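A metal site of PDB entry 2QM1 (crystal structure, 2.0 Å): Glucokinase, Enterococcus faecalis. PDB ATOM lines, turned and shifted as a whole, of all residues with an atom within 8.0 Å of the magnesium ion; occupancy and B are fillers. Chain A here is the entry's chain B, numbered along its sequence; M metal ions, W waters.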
ATOM      1  N   THR A  75      29.946  -4.474 -16.771  1.00  0.00           N
ATOM      2  CA  THR A  75      29.370  -5.805 -16.862  1.00  0.00           C
ATOM      3  C   THR A  75      28.107  -5.872 -16.010  1.00  0.00           C
ATOM      4  O   THR A  75      28.031  -5.228 -14.947  1.00  0.00           O
ATOM      5  CB  THR A  75      30.345  -6.892 -16.322  1.00  0.00           C
ATOM      6  OG1 THR A  75      29.694  -8.189 -16.346  1.00  0.00           O
ATOM      7  CG2 THR A  75      30.761  -6.567 -14.908  1.00  0.00           C
ATOM      8  N   GLY A  77      25.789  -7.627 -13.243  1.00  0.00           N
ATOM      9  CA  GLY A  77      26.099  -8.283 -11.955  1.00  0.00           C
ATOM     10  C   GLY A  77      26.887  -7.429 -10.998  1.00  0.00           C
ATOM     11  O   GLY A  77      27.080  -6.244 -11.214  1.00  0.00           O
ATOM     12  N   SER A  78      27.394  -8.037  -9.923  1.00  0.00           N
ATOM     13  CA  SER A  78      28.109  -7.234  -8.957  1.00  0.00           C
ATOM     14  C   SER A  78      29.631  -7.496  -8.981  1.00  0.00           C
ATOM     15  O   SER A  78      30.095  -8.608  -9.221  1.00  0.00           O
ATOM     16  CB  SER A  78      27.457  -7.303  -7.581  1.00  0.00           C
ATOM     17  OG  SER A  78      28.221  -8.036  -6.677  1.00  0.00           O
ATOM     18  N   ASP A 115      33.749  -2.719 -13.822  1.00  0.00           N
ATOM     19  CA  ASP A 115      32.760  -2.263 -12.863  1.00  0.00           C
ATOM     20  C   ASP A 115      31.373  -2.690 -13.305  1.00  0.00           C
ATOM     21  O   ASP A 115      31.214  -3.247 -14.367  1.00  0.00           O
ATOM     22  CB  ASP A 115      32.873  -0.734 -12.528  1.00  0.00           C
ATOM     23  CG  ASP A 115      32.447  -0.405 -11.071  1.00  0.00           C
ATOM     24  OD1 ASP A 115      31.394  -0.946 -10.554  1.00  0.00           O
ATOM     25  OD2 ASP A 115      33.197   0.360 -10.429  1.00  0.00           O
ATOM     26  N   ASN A 116      30.402  -2.499 -12.452  1.00  0.00           N
ATOM     27  CA  ASN A 116      29.017  -2.811 -12.808  1.00  0.00           C
ATOM     28  C   ASN A 116      28.557  -1.917 -13.976  1.00  0.00           C
ATOM     29  O   ASN A 116      29.015  -0.789 -14.109  1.00  0.00           O
ATOM     30  CB  ASN A 116      28.152  -2.604 -11.590  1.00  0.00           C
ATOM     31  CG  ASN A 116      26.716  -2.516 -11.931  1.00  0.00           C
ATOM     32  OD1 ASN A 116      26.066  -3.538 -12.124  1.00  0.00           O
ATOM     33  ND2 ASN A 116      26.231  -1.325 -12.111  1.00  0.00           N
ATOM     34  N   ASP A 117      27.616  -2.406 -14.783  1.00  0.00           N
ATOM     35  CA  ASP A 117      27.261  -1.724 -16.023  1.00  0.00           C
ATOM     36  C   ASP A 117      26.587  -0.359 -15.840  1.00  0.00           C
ATOM     37  O   ASP A 117      26.965   0.586 -16.512  1.00  0.00           O
ATOM     38  CB  ASP A 117      26.465  -2.642 -16.960  1.00  0.00           C
ATOM     39  CG  ASP A 117      25.148  -3.171 -16.345  1.00  0.00           C
ATOM     40  OD1 ASP A 117      24.927  -3.007 -15.126  1.00  0.00           O
ATOM     41  OD2 ASP A 117      24.358  -3.811 -17.093  1.00  0.00           O
ATOM     42  N   ALA A 118      25.650  -0.225 -14.898  1.00  0.00           N
ATOM     43  CA  ALA A 118      25.106   1.115 -14.595  1.00  0.00           C
ATOM     44  C   ALA A 118      26.099   1.997 -13.854  1.00  0.00           C
ATOM     45  O   ALA A 118      26.067   3.194 -14.011  1.00  0.00           O
ATOM     46  CB  ALA A 118      23.805   1.045 -13.878  1.00  0.00           C
ATOM     47  N   ASN A 119      27.020   1.391 -13.089  1.00  0.00           N
ATOM     48  CA  ASN A 119      28.035   2.193 -12.390  1.00  0.00           C
ATOM     49  C   ASN A 119      28.886   2.986 -13.377  1.00  0.00           C
ATOM     50  O   ASN A 119      29.114   4.178 -13.247  1.00  0.00           O
ATOM     51  CB  ASN A 119      28.928   1.308 -11.518  1.00  0.00           C
ATOM     52  CG  ASN A 119      28.259   0.937 -10.211  1.00  0.00           C
ATOM     53  OD1 ASN A 119      27.058   1.216 -10.023  1.00  0.00           O
ATOM     54  ND2 ASN A 119      28.993   0.285  -9.312  1.00  0.00           N
ATOM     55  N   VAL A 120      29.306   2.267 -14.387  1.00  0.00           N
ATOM     56  CA  VAL A 120      30.187   2.767 -15.441  1.00  0.00           C
ATOM     57  C   VAL A 120      29.429   3.787 -16.325  1.00  0.00           C
ATOM     58  O   VAL A 120      29.927   4.847 -16.640  1.00  0.00           O
ATOM     59  CB  VAL A 120      30.728   1.477 -16.138  1.00  0.00           C
ATOM     60  CG1 VAL A 120      30.539   1.441 -17.548  1.00  0.00           C
ATOM     61  CG2 VAL A 120      32.097   1.092 -15.628  1.00  0.00           C
ATOM     62  N   ALA A 121      28.187   3.488 -16.652  1.00  0.00           N
ATOM     63  CA  ALA A 121      27.326   4.469 -17.312  1.00  0.00           C
ATOM     64  C   ALA A 121      27.179   5.779 -16.515  1.00  0.00           C
ATOM     65  O   ALA A 121      27.283   6.866 -17.072  1.00  0.00           O
ATOM     66  CB  ALA A 121      25.953   3.841 -17.625  1.00  0.00           C
ATOM     67  N   ALA A 122      27.022   5.649 -15.199  1.00  0.00           N
ATOM     68  CA  ALA A 122      27.052   6.759 -14.282  1.00  0.00           C
ATOM     69  C   ALA A 122      28.338   7.562 -14.417  1.00  0.00           C
ATOM     70  O   ALA A 122      28.284   8.786 -14.434  1.00  0.00           O
ATOM     71  CB  ALA A 122      26.876   6.222 -12.802  1.00  0.00           C
ATOM     72  N   PHE A 139      23.061   8.376 -11.035  1.00  0.00           N
ATOM     73  CA  PHE A 139      22.539   7.903 -12.326  1.00  0.00           C
ATOM     74  C   PHE A 139      21.506   6.799 -12.106  1.00  0.00           C
ATOM     75  O   PHE A 139      21.767   5.825 -11.390  1.00  0.00           O
ATOM     76  CB  PHE A 139      23.673   7.411 -13.249  1.00  0.00           C
ATOM     77  CG  PHE A 139      23.206   6.988 -14.617  1.00  0.00           C
ATOM     78  CD1 PHE A 139      22.586   7.902 -15.467  1.00  0.00           C
ATOM     79  CD2 PHE A 139      23.390   5.690 -15.060  1.00  0.00           C
ATOM     80  CE1 PHE A 139      22.140   7.540 -16.721  1.00  0.00           C
ATOM     81  CE2 PHE A 139      22.938   5.299 -16.342  1.00  0.00           C
ATOM     82  CZ  PHE A 139      22.303   6.242 -17.156  1.00  0.00           C
ATOM     83  N   THR A 141      19.070   4.346 -14.636  1.00  0.00           N
ATOM     84  CA  THR A 141      18.761   3.925 -15.999  1.00  0.00           C
ATOM     85  C   THR A 141      17.517   3.047 -16.067  1.00  0.00           C
ATOM     86  O   THR A 141      17.411   2.034 -15.383  1.00  0.00           O
ATOM     87  CB  THR A 141      19.966   3.277 -16.694  1.00  0.00           C
ATOM     88  OG1 THR A 141      19.618   2.862 -18.034  1.00  0.00           O
ATOM     89  CG2 THR A 141      20.482   2.110 -15.890  1.00  0.00           C
ATOM     90  N   VAL A 146      15.884  -1.847 -14.137  1.00  0.00           N
ATOM     91  CA  VAL A 146      16.217  -0.536 -13.610  1.00  0.00           C
ATOM     92  C   VAL A 146      17.570  -0.636 -12.882  1.00  0.00           C
ATOM     93  O   VAL A 146      17.759  -1.510 -12.045  1.00  0.00           O
ATOM     94  CB  VAL A 146      15.075   0.066 -12.756  1.00  0.00           C
ATOM     95  CG1 VAL A 146      15.482   1.392 -12.166  1.00  0.00           C
ATOM     96  CG2 VAL A 146      13.880   0.287 -13.608  1.00  0.00           C
ATOM     97  N   GLY A 147      18.505   0.242 -13.255  1.00  0.00           N
ATOM     98  CA  GLY A 147      19.887   0.148 -12.730  1.00  0.00           C
ATOM     99  C   GLY A 147      20.291   1.522 -12.245  1.00  0.00           C
ATOM    100  O   GLY A 147      19.536   2.503 -12.379  1.00  0.00           O
ATOM    101  N   GLY A 148      21.431   1.608 -11.603  1.00  0.00           N
ATOM    102  CA  GLY A 148      21.909   2.906 -11.218  1.00  0.00           C
ATOM    103  C   GLY A 148      23.350   2.914 -10.744  1.00  0.00           C
ATOM    104  O   GLY A 148      23.955   1.852 -10.465  1.00  0.00           O
ATOM    105  N   GLY A 149      23.898   4.139 -10.673  1.00  0.00           N
ATOM    106  CA  GLY A 149      25.244   4.356 -10.153  1.00  0.00           C
ATOM    107  C   GLY A 149      25.218   5.619  -9.306  1.00  0.00           C
ATOM    108  O   GLY A 149      24.494   6.577  -9.623  1.00  0.00           O
ATOM    109  N   ILE A 150      25.986   5.567  -8.216  1.00  0.00           N
ATOM    110  CA  ILE A 150      26.156   6.685  -7.279  1.00  0.00           C
ATOM    111  C   ILE A 150      27.582   7.126  -7.135  1.00  0.00           C
ATOM    112  O   ILE A 150      28.456   6.373  -6.719  1.00  0.00           O
ATOM    113  CB  ILE A 150      25.596   6.313  -5.847  1.00  0.00           C
ATOM    114  CG1 ILE A 150      24.102   5.928  -5.954  1.00  0.00           C
ATOM    115  CG2 ILE A 150      25.896   7.507  -4.931  1.00  0.00           C
ATOM    116  CD1 ILE A 150      23.276   5.488  -4.621  1.00  0.00           C
ATOM    117  N   LEU A 156      32.828   6.730  -6.919  1.00  0.00           N
ATOM    118  CA  LEU A 156      31.748   5.849  -7.268  1.00  0.00           C
ATOM    119  C   LEU A 156      31.494   4.947  -6.031  1.00  0.00           C
ATOM    120  O   LEU A 156      32.446   4.455  -5.465  1.00  0.00           O
ATOM    121  CB  LEU A 156      32.193   4.995  -8.434  1.00  0.00           C
ATOM    122  CG  LEU A 156      31.293   4.555  -9.589  1.00  0.00           C
ATOM    123  CD1 LEU A 156      31.888   3.192 -10.045  1.00  0.00           C
ATOM    124  CD2 LEU A 156      29.755   4.506  -9.327  1.00  0.00           C
ATOM    125  N   LEU A 157      30.252   4.760  -5.619  1.00  0.00           N
ATOM    126  CA  LEU A 157      29.985   3.812  -4.473  1.00  0.00           C
ATOM    127  C   LEU A 157      29.737   2.316  -4.832  1.00  0.00           C
ATOM    128  O   LEU A 157      29.046   2.005  -5.795  1.00  0.00           O
ATOM    129  CB  LEU A 157      28.900   4.308  -3.532  1.00  0.00           C
ATOM    130  CG  LEU A 157      29.007   5.792  -3.102  1.00  0.00           C
ATOM    131  CD1 LEU A 157      27.939   6.096  -2.178  1.00  0.00           C
ATOM    132  CD2 LEU A 157      30.370   6.126  -2.453  1.00  0.00           C
ATOM    133  N   HIS A 158      30.306   1.410  -4.031  1.00  0.00           N
ATOM    134  CA  HIS A 158      30.169  -0.020  -4.236  1.00  0.00           C
ATOM    135  C   HIS A 158      29.515  -0.686  -3.039  1.00  0.00           C
ATOM    136  O   HIS A 158      28.822  -1.647  -3.196  1.00  0.00           O
ATOM    137  CB  HIS A 158      31.548  -0.629  -4.567  1.00  0.00           C
ATOM    138  CG  HIS A 158      32.135  -0.034  -5.818  1.00  0.00           C
ATOM    139  ND1 HIS A 158      32.907   1.106  -5.821  1.00  0.00           N
ATOM    140  CD2 HIS A 158      31.913  -0.342  -7.124  1.00  0.00           C
ATOM    141  CE1 HIS A 158      33.203   1.443  -7.073  1.00  0.00           C
ATOM    142  NE2 HIS A 158      32.613   0.575  -7.878  1.00  0.00           N
ATOM    143  N   GLY A 162      29.366  -4.975  -3.258  1.00  0.00           N
ATOM    144  CA  GLY A 162      29.225  -4.458  -4.588  1.00  0.00           C
ATOM    145  C   GLY A 162      27.803  -4.111  -5.030  1.00  0.00           C
ATOM    146  O   GLY A 162      27.536  -4.062  -6.244  1.00  0.00           O
ATOM    147  N   CYS A 163      26.907  -3.815  -4.086  1.00  0.00           N
ATOM    148  CA  CYS A 163      25.474  -3.620  -4.461  1.00  0.00           C
ATOM    149  C   CYS A 163      24.959  -2.212  -4.337  1.00  0.00           C
ATOM    150  O   CYS A 163      23.730  -1.942  -4.546  1.00  0.00           O
ATOM    151  CB  CYS A 163      24.550  -4.532  -3.669  1.00  0.00           C
ATOM    152  SG  CYS A 163      24.626  -6.243  -4.124  1.00  0.00           S
ATOM    153  N   ALA A 164      25.878  -1.278  -4.017  1.00  0.00           N
ATOM    154  CA  ALA A 164      25.536   0.109  -3.940  1.00  0.00           C
ATOM    155  C   ALA A 164      25.071   0.502  -5.300  1.00  0.00           C
ATOM    156  O   ALA A 164      25.636   0.043  -6.295  1.00  0.00           O
ATOM    157  CB  ALA A 164      26.782   0.973  -3.551  1.00  0.00           C
ATOM    158  N   GLY A 165      24.086   1.395  -5.357  1.00  0.00           N
ATOM    159  CA  GLY A 165      23.578   1.802  -6.636  1.00  0.00           C
ATOM    160  C   GLY A 165      22.382   1.042  -7.186  1.00  0.00           C
ATOM    161  O   GLY A 165      21.835   1.421  -8.233  1.00  0.00           O
ATOM    162  N   GLU A 166      21.942   0.006  -6.495  1.00  0.00           N
ATOM    163  CA  GLU A 166      20.863  -0.823  -6.979  1.00  0.00           C
ATOM    164  C   GLU A 166      19.468  -0.199  -6.776  1.00  0.00           C
ATOM    165  O   GLU A 166      18.598  -0.792  -6.140  1.00  0.00           O
ATOM    166  CB  GLU A 166      20.966  -2.234  -6.405  1.00  0.00           C
ATOM    167  CG  GLU A 166      22.121  -3.065  -7.036  1.00  0.00           C
ATOM    168  CD  GLU A 166      21.927  -3.258  -8.566  1.00  0.00           C
ATOM    169  OE1 GLU A 166      22.918  -3.182  -9.314  1.00  0.00           O
ATOM    170  OE2 GLU A 166      20.776  -3.452  -9.031  1.00  0.00           O
ATOM    171  N   VAL A 167      19.249   0.982  -7.282  1.00  0.00           N
ATOM    172  CA  VAL A 167      17.962   1.673  -6.949  1.00  0.00           C
ATOM    173  C   VAL A 167      16.694   1.059  -7.559  1.00  0.00           C
ATOM    174  O   VAL A 167      15.574   1.455  -7.226  1.00  0.00           O
ATOM    175  CB  VAL A 167      18.040   3.161  -7.275  1.00  0.00           C
ATOM    176  CG1 VAL A 167      19.271   3.787  -6.536  1.00  0.00           C
ATOM    177  CG2 VAL A 167      18.172   3.356  -8.776  1.00  0.00           C
HETATM  178 MG    MG M   1      25.174   0.020 -10.443  1.00  0.00          MG
HETATM  179  O   HOH W   1      25.082  -1.547  -8.647  1.00  0.00           O
HETATM  180  O   HOH W   2      22.698  -1.055 -11.059  1.00  0.00           O
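Merely in contact with the magnesium ion: Ala 118 (3.8 Å).
Within 4 Å of the magnesium ion: Asn 116, Ala 118, Asn 119 and Gly 148.
Along chain A the residues within 4 Å of the magnesium ion span positions 116 to 148.
The backbone NH (N) of Gly 148 lies close to the backbone carbonyl oxygen (O) of Gly 165 (3.4 Å).
OD1 of Asp 115 sits at hydrogen-bond distance from ND2 of Asn 119 (3.0 Å).
The side-chain amide nitrogen (ND2) of Asn 116 lies close to the backbone NH (N) of Ala 118, 3.1 Å away.
OD1 of Asp 117 sits close to OD1 of Asn 116.
The backbone carbonyl oxygen (O) of Gly 77 lies close to the side-chain amide oxygen (OD1) of Asn 116 (3.0 Å).
The magnesium ion is bound by O of Gly 148 (2.2 Å), OD1 of Asn 119 (2.3 Å), water W1 (2.4 Å) and ND2 of Asn 116 (2.4 Å).
Slightly farther from the magnesium ion lies water W2 (2.8 Å).
Water W1 lies within hydrogen-bond range of OE1 of Glu 166 and O of Ala 164.
Water W2 bridges OE1 of Glu 166 and N of Gly 148.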
